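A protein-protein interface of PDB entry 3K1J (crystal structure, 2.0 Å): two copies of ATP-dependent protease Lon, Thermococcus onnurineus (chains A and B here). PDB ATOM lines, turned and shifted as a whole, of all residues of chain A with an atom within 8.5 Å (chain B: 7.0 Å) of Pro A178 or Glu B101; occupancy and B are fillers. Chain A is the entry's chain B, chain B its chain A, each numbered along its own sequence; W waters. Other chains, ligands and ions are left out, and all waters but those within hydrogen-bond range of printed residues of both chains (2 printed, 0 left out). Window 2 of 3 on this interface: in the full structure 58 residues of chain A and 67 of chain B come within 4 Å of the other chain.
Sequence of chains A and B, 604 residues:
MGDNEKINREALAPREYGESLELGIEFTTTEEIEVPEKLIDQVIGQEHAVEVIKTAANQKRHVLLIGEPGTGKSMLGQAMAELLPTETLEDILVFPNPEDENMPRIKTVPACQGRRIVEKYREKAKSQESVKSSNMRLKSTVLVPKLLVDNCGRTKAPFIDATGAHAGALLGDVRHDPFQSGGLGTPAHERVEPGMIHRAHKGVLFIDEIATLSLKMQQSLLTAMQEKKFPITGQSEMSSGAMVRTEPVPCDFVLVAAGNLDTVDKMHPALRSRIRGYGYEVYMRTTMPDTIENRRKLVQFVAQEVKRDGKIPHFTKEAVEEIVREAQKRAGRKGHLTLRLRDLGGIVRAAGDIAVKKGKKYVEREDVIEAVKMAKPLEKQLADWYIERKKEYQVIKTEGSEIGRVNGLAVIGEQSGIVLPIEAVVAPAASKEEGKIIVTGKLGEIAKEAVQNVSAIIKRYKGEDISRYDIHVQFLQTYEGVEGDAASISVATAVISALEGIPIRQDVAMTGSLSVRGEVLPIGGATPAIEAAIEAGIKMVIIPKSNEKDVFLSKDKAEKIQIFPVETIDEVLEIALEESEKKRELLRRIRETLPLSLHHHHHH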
ATOM      1  N   ARG A 175     -20.012  32.547  10.565  1.00  0.00           N
ATOM      2  CA  ARG A 175     -20.453  31.722  11.680  1.00  0.00           C
ATOM      3  C   ARG A 175     -19.472  31.758  12.836  1.00  0.00           C
ATOM      4  O   ARG A 175     -18.262  31.876  12.642  1.00  0.00           O
ATOM      5  CB  ARG A 175     -20.655  30.275  11.229  1.00  0.00           C
ATOM      6  CG  ARG A 175     -21.548  30.114  10.007  1.00  0.00           C
ATOM      7  CD  ARG A 175     -22.090  28.677   9.898  1.00  0.00           C
ATOM      8  NE  ARG A 175     -21.056  27.659  10.094  1.00  0.00           N
ATOM      9  CZ  ARG A 175     -20.341  27.109   9.116  1.00  0.00           C
ATOM     10  NH1 ARG A 175     -20.541  27.469   7.853  1.00  0.00           N
ATOM     11  NH2 ARG A 175     -19.425  26.195   9.402  1.00  0.00           N
ATOM     12  N   HIS A 176     -20.009  31.671  14.045  1.00  0.00           N
ATOM     13  CA  HIS A 176     -19.191  31.666  15.249  1.00  0.00           C
ATOM     14  C   HIS A 176     -18.490  30.314  15.363  1.00  0.00           C
ATOM     15  O   HIS A 176     -19.019  29.297  14.922  1.00  0.00           O
ATOM     16  CB  HIS A 176     -20.081  31.893  16.476  1.00  0.00           C
ATOM     17  CG  HIS A 176     -19.359  31.768  17.780  1.00  0.00           C
ATOM     18  ND1 HIS A 176     -19.720  30.852  18.746  1.00  0.00           N
ATOM     19  CD2 HIS A 176     -18.295  32.440  18.280  1.00  0.00           C
ATOM     20  CE1 HIS A 176     -18.909  30.965  19.783  1.00  0.00           C
ATOM     21  NE2 HIS A 176     -18.035  31.921  19.524  1.00  0.00           N
ATOM     22  N   ASP A 177     -17.301  30.311  15.952  1.00  0.00           N
ATOM     23  CA  ASP A 177     -16.534  29.081  16.144  1.00  0.00           C
ATOM     24  C   ASP A 177     -16.081  29.027  17.600  1.00  0.00           C
ATOM     25  O   ASP A 177     -15.287  29.856  18.042  1.00  0.00           O
ATOM     26  CB  ASP A 177     -15.318  29.062  15.208  1.00  0.00           C
ATOM     27  CG  ASP A 177     -14.510  27.769  15.309  1.00  0.00           C
ATOM     28  OD1 ASP A 177     -15.051  26.744  15.785  1.00  0.00           O
ATOM     29  OD2 ASP A 177     -13.328  27.779  14.891  1.00  0.00           O
ATOM     30  N   PRO A 178     -16.604  28.063  18.373  1.00  0.00           N
ATOM     31  CA  PRO A 178     -16.224  27.936  19.784  1.00  0.00           C
ATOM     32  C   PRO A 178     -14.730  27.668  19.934  1.00  0.00           C
ATOM     33  O   PRO A 178     -14.125  28.007  20.951  1.00  0.00           O
ATOM     34  CB  PRO A 178     -17.068  26.759  20.264  1.00  0.00           C
ATOM     35  CG  PRO A 178     -18.287  26.841  19.394  1.00  0.00           C
ATOM     36  CD  PRO A 178     -17.682  27.116  18.038  1.00  0.00           C
ATOM     37  N   PHE A 179     -14.148  27.062  18.902  1.00  0.00           N
ATOM     38  CA  PHE A 179     -12.728  26.723  18.878  1.00  0.00           C
ATOM     39  C   PHE A 179     -11.928  27.721  18.040  1.00  0.00           C
ATOM     40  O   PHE A 179     -11.520  28.777  18.526  1.00  0.00           O
ATOM     41  CB  PHE A 179     -12.548  25.314  18.303  1.00  0.00           C
ATOM     42  CG  PHE A 179     -11.907  24.345  19.257  1.00  0.00           C
ATOM     43  CD1 PHE A 179     -12.438  24.144  20.531  1.00  0.00           C
ATOM     44  CD2 PHE A 179     -10.778  23.620  18.877  1.00  0.00           C
ATOM     45  CE1 PHE A 179     -11.853  23.235  21.416  1.00  0.00           C
ATOM     46  CE2 PHE A 179     -10.185  22.707  19.755  1.00  0.00           C
ATOM     47  CZ  PHE A 179     -10.724  22.515  21.027  1.00  0.00           C
ATOM     48  N   GLY A 185     -11.220  23.670  15.658  1.00  0.00           N
ATOM     49  CA  GLY A 185     -11.791  24.864  15.060  1.00  0.00           C
ATOM     50  C   GLY A 185     -12.041  24.704  13.572  1.00  0.00           C
ATOM     51  O   GLY A 185     -11.381  23.895  12.911  1.00  0.00           O
ATOM     52  N   THR A 186     -12.994  25.468  13.040  1.00  0.00           N
ATOM     53  CA  THR A 186     -13.325  25.405  11.615  1.00  0.00           C
ATOM     54  C   THR A 186     -12.685  26.565  10.854  1.00  0.00           C
ATOM     55  O   THR A 186     -12.685  27.705  11.325  1.00  0.00           O
ATOM     56  CB  THR A 186     -14.854  25.441  11.391  1.00  0.00           C
ATOM     57  OG1 THR A 186     -15.442  24.256  11.944  1.00  0.00           O
ATOM     58  CG2 THR A 186     -15.177  25.517   9.901  1.00  0.00           C
ATOM     59  N   ARG A 191     -16.634  29.341   7.103  1.00  0.00           N
ATOM     60  CA  ARG A 191     -17.679  29.903   7.947  1.00  0.00           C
ATOM     61  C   ARG A 191     -18.315  31.164   7.372  1.00  0.00           C
ATOM     62  O   ARG A 191     -19.217  31.742   7.970  1.00  0.00           O
ATOM     63  CB  ARG A 191     -17.104  30.192   9.336  1.00  0.00           C
ATOM     64  CG  ARG A 191     -16.733  28.920  10.086  1.00  0.00           C
ATOM     65  CD  ARG A 191     -16.247  29.190  11.495  1.00  0.00           C
ATOM     66  NE  ARG A 191     -14.855  29.634  11.547  1.00  0.00           N
ATOM     67  CZ  ARG A 191     -14.461  30.816  12.009  1.00  0.00           C
ATOM     68  NH1 ARG A 191     -15.355  31.685  12.454  1.00  0.00           N
ATOM     69  NH2 ARG A 191     -13.167  31.117  12.057  1.00  0.00           N
ATOM     70  N   SER A 239     -19.987  37.042  18.760  1.00  0.00           N
ATOM     71  CA  SER A 239     -19.453  35.947  17.945  1.00  0.00           C
ATOM     72  C   SER A 239     -17.997  36.122  17.531  1.00  0.00           C
ATOM     73  O   SER A 239     -17.535  37.245  17.312  1.00  0.00           O
ATOM     74  CB  SER A 239     -20.313  35.796  16.682  1.00  0.00           C
ATOM     75  OG  SER A 239     -19.780  34.841  15.779  1.00  0.00           O
ATOM     76  N   SER A 240     -17.285  35.004  17.408  1.00  0.00           N
ATOM     77  CA  SER A 240     -15.891  35.042  16.978  1.00  0.00           C
ATOM     78  C   SER A 240     -15.858  35.382  15.483  1.00  0.00           C
ATOM     79  O   SER A 240     -14.806  35.690  14.932  1.00  0.00           O
ATOM     80  CB  SER A 240     -15.204  33.690  17.228  1.00  0.00           C
ATOM     81  OG  SER A 240     -15.774  32.651  16.442  1.00  0.00           O
ATOM     82  N   GLY A 241     -17.018  35.321  14.832  1.00  0.00           N
ATOM     83  CA  GLY A 241     -17.084  35.650  13.420  1.00  0.00           C
ATOM     84  C   GLY A 241     -16.749  37.117  13.195  1.00  0.00           C
ATOM     85  O   GLY A 241     -16.344  37.513  12.097  1.00  0.00           O
ATOM     86  N   PHE B  95     -33.145  20.580  17.866  1.00  0.00           N
ATOM     87  CA  PHE B  95     -31.976  19.735  18.115  1.00  0.00           C
ATOM     88  C   PHE B  95     -30.682  20.527  18.004  1.00  0.00           C
ATOM     89  O   PHE B  95     -30.653  21.612  17.427  1.00  0.00           O
ATOM     90  CB  PHE B  95     -31.889  18.621  17.066  1.00  0.00           C
ATOM     91  CG  PHE B  95     -32.870  17.500  17.255  1.00  0.00           C
ATOM     92  CD1 PHE B  95     -32.423  16.235  17.626  1.00  0.00           C
ATOM     93  CD2 PHE B  95     -34.226  17.684  16.999  1.00  0.00           C
ATOM     94  CE1 PHE B  95     -33.312  15.164  17.735  1.00  0.00           C
ATOM     95  CE2 PHE B  95     -35.127  16.613  17.106  1.00  0.00           C
ATOM     96  CZ  PHE B  95     -34.664  15.353  17.472  1.00  0.00           C
ATOM     97  N   PRO B  96     -29.586  19.986  18.554  1.00  0.00           N
ATOM     98  CA  PRO B  96     -28.309  20.691  18.457  1.00  0.00           C
ATOM     99  C   PRO B  96     -27.811  20.491  17.027  1.00  0.00           C
ATOM    100  O   PRO B  96     -28.117  19.471  16.407  1.00  0.00           O
ATOM    101  CB  PRO B  96     -27.437  19.967  19.478  1.00  0.00           C
ATOM    102  CG  PRO B  96     -27.962  18.572  19.429  1.00  0.00           C
ATOM    103  CD  PRO B  96     -29.465  18.802  19.423  1.00  0.00           C
ATOM    104  N   ASN B  97     -27.074  21.461  16.497  1.00  0.00           N
ATOM    105  CA  ASN B  97     -26.536  21.359  15.140  1.00  0.00           C
ATOM    106  C   ASN B  97     -25.019  21.164  15.230  1.00  0.00           C
ATOM    107  O   ASN B  97     -24.282  22.102  15.526  1.00  0.00           O
ATOM    108  CB  ASN B  97     -26.843  22.630  14.346  1.00  0.00           C
ATOM    109  CG  ASN B  97     -26.448  22.512  12.890  1.00  0.00           C
ATOM    110  OD1 ASN B  97     -25.505  21.792  12.547  1.00  0.00           O
ATOM    111  ND2 ASN B  97     -27.156  23.231  12.024  1.00  0.00           N
ATOM    112  N   PRO B  98     -24.537  19.937  14.981  1.00  0.00           N
ATOM    113  CA  PRO B  98     -23.106  19.611  15.036  1.00  0.00           C
ATOM    114  C   PRO B  98     -22.241  20.485  14.130  1.00  0.00           C
ATOM    115  O   PRO B  98     -21.113  20.834  14.477  1.00  0.00           O
ATOM    116  CB  PRO B  98     -23.066  18.145  14.599  1.00  0.00           C
ATOM    117  CG  PRO B  98     -24.401  17.624  15.023  1.00  0.00           C
ATOM    118  CD  PRO B  98     -25.327  18.747  14.621  1.00  0.00           C
ATOM    119  N   GLU B  99     -22.788  20.830  12.970  1.00  0.00           N
ATOM    120  CA  GLU B  99     -22.090  21.637  11.978  1.00  0.00           C
ATOM    121  C   GLU B  99     -22.122  23.145  12.206  1.00  0.00           C
ATOM    122  O   GLU B  99     -21.291  23.869  11.667  1.00  0.00           O
ATOM    123  CB  GLU B  99     -22.675  21.347  10.603  1.00  0.00           C
ATOM    124  CG  GLU B  99     -22.361  19.962  10.088  1.00  0.00           C
ATOM    125  CD  GLU B  99     -23.371  19.488   9.065  1.00  0.00           C
ATOM    126  OE1 GLU B  99     -23.694  20.264   8.136  1.00  0.00           O
ATOM    127  OE2 GLU B  99     -23.840  18.335   9.195  1.00  0.00           O
ATOM    128  N   ASP B 100     -23.083  23.620  12.988  1.00  0.00           N
ATOM    129  CA  ASP B 100     -23.219  25.053  13.238  1.00  0.00           C
ATOM    130  C   ASP B 100     -24.053  25.249  14.500  1.00  0.00           C
ATOM    131  O   ASP B 100     -25.276  25.381  14.432  1.00  0.00           O
ATOM    132  CB  ASP B 100     -23.902  25.699  12.029  1.00  0.00           C
ATOM    133  CG  ASP B 100     -24.014  27.206  12.147  1.00  0.00           C
ATOM    134  OD1 ASP B 100     -23.477  27.778  13.116  1.00  0.00           O
ATOM    135  OD2 ASP B 100     -24.641  27.818  11.256  1.00  0.00           O
ATOM    136  N   GLU B 101     -23.392  25.278  15.650  1.00  0.00           N
ATOM    137  CA  GLU B 101     -24.112  25.417  16.904  1.00  0.00           C
ATOM    138  C   GLU B 101     -25.100  26.574  16.987  1.00  0.00           C
ATOM    139  O   GLU B 101     -26.119  26.458  17.670  1.00  0.00           O
ATOM    140  CB  GLU B 101     -23.166  25.532  18.093  1.00  0.00           C
ATOM    141  CG  GLU B 101     -23.937  25.345  19.393  1.00  0.00           C
ATOM    142  CD  GLU B 101     -23.148  25.692  20.621  1.00  0.00           C
ATOM    143  OE1 GLU B 101     -21.896  25.718  20.540  1.00  0.00           O
ATOM    144  OE2 GLU B 101     -23.787  25.928  21.673  1.00  0.00           O
ATOM    145  N   ASN B 102     -24.803  27.687  16.318  1.00  0.00           N
ATOM    146  CA  ASN B 102     -25.702  28.834  16.367  1.00  0.00           C
ATOM    147  C   ASN B 102     -26.922  28.737  15.452  1.00  0.00           C
ATOM    148  O   ASN B 102     -27.689  29.688  15.335  1.00  0.00           O
ATOM    149  CB  ASN B 102     -24.937  30.132  16.099  1.00  0.00           C
ATOM    150  CG  ASN B 102     -24.168  30.616  17.320  1.00  0.00           C
ATOM    151  OD1 ASN B 102     -24.399  30.154  18.443  1.00  0.00           O
ATOM    152  ND2 ASN B 102     -23.264  31.566  17.111  1.00  0.00           N
ATOM    153  N   MET B 103     -27.089  27.599  14.786  1.00  0.00           N
ATOM    154  CA  MET B 103     -28.269  27.391  13.954  1.00  0.00           C
ATOM    155  C   MET B 103     -28.907  26.054  14.327  1.00  0.00           C
ATOM    156  O   MET B 103     -28.851  25.084  13.570  1.00  0.00           O
ATOM    157  CB  MET B 103     -27.957  27.388  12.457  1.00  0.00           C
ATOM    158  CG  MET B 103     -29.247  27.308  11.645  1.00  0.00           C
ATOM    159  SD  MET B 103     -29.096  27.253   9.854  1.00  0.00           S
ATOM    160  CE  MET B 103     -28.864  25.506   9.608  1.00  0.00           C
ATOM    161  N   PRO B 104     -29.503  25.985  15.520  1.00  0.00           N
ATOM    162  CA  PRO B 104     -30.156  24.758  15.994  1.00  0.00           C
ATOM    163  C   PRO B 104     -31.111  24.215  14.936  1.00  0.00           C
ATOM    164  O   PRO B 104     -31.768  24.978  14.227  1.00  0.00           O
ATOM    165  CB  PRO B 104     -30.895  25.226  17.238  1.00  0.00           C
ATOM    166  CG  PRO B 104     -29.976  26.303  17.784  1.00  0.00           C
ATOM    167  CD  PRO B 104     -29.570  27.052  16.532  1.00  0.00           C
ATOM    168  N   ARG B 105     -31.186  22.897  14.821  1.00  0.00           N
ATOM    169  CA  ARG B 105     -32.074  22.317  13.831  1.00  0.00           C
ATOM    170  C   ARG B 105     -33.484  22.058  14.360  1.00  0.00           C
ATOM    171  O   ARG B 105     -33.689  21.839  15.553  1.00  0.00           O
ATOM    172  CB  ARG B 105     -31.413  21.081  13.219  1.00  0.00           C
ATOM    173  CG  ARG B 105     -30.530  21.536  12.049  1.00  0.00           C
ATOM    174  CD  ARG B 105     -29.298  20.700  11.783  1.00  0.00           C
ATOM    175  NE  ARG B 105     -29.558  19.441  11.085  1.00  0.00           N
ATOM    176  CZ  ARG B 105     -30.311  19.307   9.991  1.00  0.00           C
ATOM    177  NH1 ARG B 105     -30.912  20.360   9.448  1.00  0.00           N
ATOM    178  NH2 ARG B 105     -30.437  18.113   9.420  1.00  0.00           N
ATOM    179  N   ASP B 177     -26.201  33.395  27.564  1.00  0.00           N
ATOM    180  CA  ASP B 177     -25.392  32.372  28.209  1.00  0.00           C
ATOM    181  C   ASP B 177     -24.242  33.045  28.960  1.00  0.00           C
ATOM    182  O   ASP B 177     -23.321  33.594  28.355  1.00  0.00           O
ATOM    183  CB  ASP B 177     -24.825  31.388  27.187  1.00  0.00           C
ATOM    184  CG  ASP B 177     -24.083  30.234  27.844  1.00  0.00           C
ATOM    185  OD1 ASP B 177     -23.958  30.229  29.088  1.00  0.00           O
ATOM    186  OD2 ASP B 177     -23.622  29.326  27.123  1.00  0.00           O
ATOM    187  N   GLY B 185     -20.556  26.446  28.763  1.00  0.00           N
ATOM    188  CA  GLY B 185     -21.905  26.963  28.921  1.00  0.00           C
ATOM    189  C   GLY B 185     -23.035  26.019  28.557  1.00  0.00           C
ATOM    190  O   GLY B 185     -22.881  24.797  28.584  1.00  0.00           O
ATOM    191  N   THR B 186     -24.181  26.599  28.219  1.00  0.00           N
ATOM    192  CA  THR B 186     -25.358  25.830  27.853  1.00  0.00           C
ATOM    193  C   THR B 186     -25.533  25.770  26.340  1.00  0.00           C
ATOM    194  O   THR B 186     -25.422  26.787  25.662  1.00  0.00           O
ATOM    195  CB  THR B 186     -26.622  26.458  28.454  1.00  0.00           C
ATOM    196  OG1 THR B 186     -26.534  26.415  29.881  1.00  0.00           O
ATOM    197  CG2 THR B 186     -27.865  25.714  28.000  1.00  0.00           C
ATOM    198  N   PRO B 187     -25.809  24.568  25.795  1.00  0.00           N
ATOM    199  CA  PRO B 187     -26.005  24.396  24.348  1.00  0.00           C
ATOM    200  C   PRO B 187     -27.051  25.400  23.856  1.00  0.00           C
ATOM    201  O   PRO B 187     -28.085  25.597  24.503  1.00  0.00           O
ATOM    202  CB  PRO B 187     -26.496  22.949  24.235  1.00  0.00           C
ATOM    203  CG  PRO B 187     -25.801  22.269  25.373  1.00  0.00           C
ATOM    204  CD  PRO B 187     -25.940  23.278  26.501  1.00  0.00           C
ATOM    205  N   ALA B 188     -26.776  26.037  22.723  1.00  0.00           N
ATOM    206  CA  ALA B 188     -27.685  27.034  22.170  1.00  0.00           C
ATOM    207  C   ALA B 188     -29.111  26.502  21.954  1.00  0.00           C
ATOM    208  O   ALA B 188     -30.087  27.221  22.164  1.00  0.00           O
ATOM    209  CB  ALA B 188     -27.117  27.579  20.847  1.00  0.00           C
ATOM    210  N   HIS B 189     -29.242  25.242  21.543  1.00  0.00           N
ATOM    211  CA  HIS B 189     -30.574  24.705  21.296  1.00  0.00           C
ATOM    212  C   HIS B 189     -31.466  24.666  22.541  1.00  0.00           C
ATOM    213  O   HIS B 189     -32.680  24.844  22.430  1.00  0.00           O
ATOM    214  CB  HIS B 189     -30.484  23.322  20.645  1.00  0.00           C
ATOM    215  CG  HIS B 189     -29.994  22.246  21.564  1.00  0.00           C
ATOM    216  ND1 HIS B 189     -30.845  21.373  22.207  1.00  0.00           N
ATOM    217  CD2 HIS B 189     -28.745  21.920  21.964  1.00  0.00           C
ATOM    218  CE1 HIS B 189     -30.139  20.553  22.965  1.00  0.00           C
ATOM    219  NE2 HIS B 189     -28.861  20.865  22.836  1.00  0.00           N
ATOM    220  N   ARG B 191     -31.544  26.849  24.843  1.00  0.00           N
ATOM    221  CA  ARG B 191     -31.795  28.218  25.280  1.00  0.00           C
ATOM    222  C   ARG B 191     -32.847  28.842  24.353  1.00  0.00           C
ATOM    223  O   ARG B 191     -33.243  29.998  24.521  1.00  0.00           O
ATOM    224  CB  ARG B 191     -30.493  29.040  25.280  1.00  0.00           C
ATOM    225  CG  ARG B 191     -29.710  28.867  26.585  1.00  0.00           C
ATOM    226  CD  ARG B 191     -28.391  29.616  26.599  1.00  0.00           C
ATOM    227  NE  ARG B 191     -27.413  29.071  25.658  1.00  0.00           N
ATOM    228  CZ  ARG B 191     -26.886  29.769  24.659  1.00  0.00           C
ATOM    229  NH1 ARG B 191     -27.252  31.026  24.472  1.00  0.00           N
ATOM    230  NH2 ARG B 191     -25.981  29.220  23.861  1.00  0.00           N
ATOM    231  N   MET B 243     -26.739  35.936  18.623  1.00  0.00           N
ATOM    232  CA  MET B 243     -26.034  35.283  17.524  1.00  0.00           C
ATOM    233  C   MET B 243     -26.620  33.921  17.153  1.00  0.00           C
ATOM    234  O   MET B 243     -26.154  33.275  16.213  1.00  0.00           O
ATOM    235  CB  MET B 243     -24.541  35.138  17.840  1.00  0.00           C
ATOM    236  CG  MET B 243     -24.194  34.249  19.026  1.00  0.00           C
ATOM    237  SD  MET B 243     -22.391  34.077  19.187  1.00  0.00           S
ATOM    238  CE  MET B 243     -22.231  32.689  20.288  1.00  0.00           C
ATOM    239  N   VAL B 244     -27.634  33.482  17.895  1.00  0.00           N
ATOM    240  CA  VAL B 244     -28.283  32.206  17.605  1.00  0.00           C
ATOM    241  C   VAL B 244     -29.526  32.467  16.739  1.00  0.00           C
ATOM    242  O   VAL B 244     -30.339  33.339  17.048  1.00  0.00           O
ATOM    243  CB  VAL B 244     -28.744  31.477  18.898  1.00  0.00           C
ATOM    244  CG1 VAL B 244     -29.483  30.197  18.527  1.00  0.00           C
ATOM    245  CG2 VAL B 244     -27.544  31.155  19.785  1.00  0.00           C
ATOM    246  N   ARG B 245     -29.650  31.722  15.648  1.00  0.00           N
ATOM    247  CA  ARG B 245     -30.790  31.860  14.759  1.00  0.00           C
ATOM    248  C   ARG B 245     -31.057  30.469  14.206  1.00  0.00           C
ATOM    249  O   ARG B 245     -30.317  29.981  13.348  1.00  0.00           O
ATOM    250  CB  ARG B 245     -30.474  32.832  13.618  1.00  0.00           C
ATOM    251  CG  ARG B 245     -31.677  33.202  12.774  1.00  0.00           C
ATOM    252  CD  ARG B 245     -31.257  33.978  11.531  1.00  0.00           C
ATOM    253  NE  ARG B 245     -32.409  34.361  10.721  1.00  0.00           N
ATOM    254  CZ  ARG B 245     -33.222  35.378  11.000  1.00  0.00           C
ATOM    255  NH1 ARG B 245     -33.007  36.129  12.081  1.00  0.00           N
ATOM    256  NH2 ARG B 245     -34.257  35.639  10.196  1.00  0.00           N
HETATM  257  O   HOH W   1     -22.673  32.197  14.436  1.00  0.00           O
HETATM  258  O   HOH W   2     -21.980  28.436  14.965  1.00  0.00           O
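Printed residues of chain A that touch a printed residue of chain B: Arg A175, His A176, Pro A178 and Ser A239.
Hydrophobic or aromatic side chains of chain A within 4 Å of the printed part of chain B: His A176 and Pro A178.
Along chain A the printed residues that touch a printed residue of chain B span positions 175 to 239.
Of the 21 printed residues of chain B, 5 touch a printed residue of chain A.
Hydrophobic or aromatic side chains of chain B within 4 Å of the printed part of chain A: Met B243.
Among the printed residues, Asp or Glu carboxylates within 4 Å of a Lys or Arg side-chain nitrogen of the other chain: Arg A175 with Asp B100 (3.8 Å).
Positions printed for both chains: 177, 185, 186 and 191.
Of the 6 pairs that touch across the chains among the printed residues, none has its exchanged pair printed and touching as well.
Water W2 lies within hydrogen-bond range of OD1 of Asp B100 (2.5 Å), O of His A176 (3.1 Å) and N of Asn B102 (3.2 Å).
Water W1 lies within hydrogen-bond range of N of His A176 (2.7 Å) and ND2 of Asn B102 (2.8 Å).
Of chain B, only Glu B101 comes within 4 Å of Pro A178.
Of chain A, only Pro A178 comes within 4 Å of Glu B101.
Printed residues of chain A within 4 Å of Met B243: His A176 and Ser A239.
Printed residues of chain A within 4 Å of Asp B100: Arg A175.
Of the printed residues of chain B, His A176 touches Asn B102 (3.3 Å) and Met B243 (3.5 Å).
Of the printed residues of chain A, Glu B99 touches Arg A175 (3.7 Å).
Of the printed residues of chain B, Ser A239 touches Met B243 (3.7 Å).
Pro B98 touches none of the printed residues of chain A.
The nearest residue of chain A that does not touch Glu B101 is His A176 (5.9 Å).
OD2 of Asp B100 is in salt-bridge range of NE of Arg A175, at 3.8 Å.
N of Asn B102 lies close to OD1 of Asp B100, 3.5 Å away.
OE2 of Glu B101 is in hydrogen-bond range of N of Ala B188 (3.2 Å).
The side-chain hydroxyl of Ser A239 is in hydrogen-bond range of the backbone NH of Gly A241 (3.0 Å).
The side-chain amide oxygen of Asn B97 is in hydrogen-bond range of the backbone NH of Asp B100 (3.1 Å).
The backbone NH (N) of Arg A175 sits at hydrogen-bond distance from the backbone carbonyl oxygen (O) of Arg A191, at 2.8 Å.
N of Arg B245 sits at hydrogen-bond distance from O of Asn B102, 2.8 Å away.
O of Glu B99 touches NH2 of Arg A175, 3.7 Å away.
His A176 touches Asn B102 (CB to ND2, 3.3 Å).
His A176 touches Met B243.
CG of Pro A178 touches OE1 of Glu B101 (3.9 Å).
Ser A239 touches Met B243 (CB to SD, 3.7 Å).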
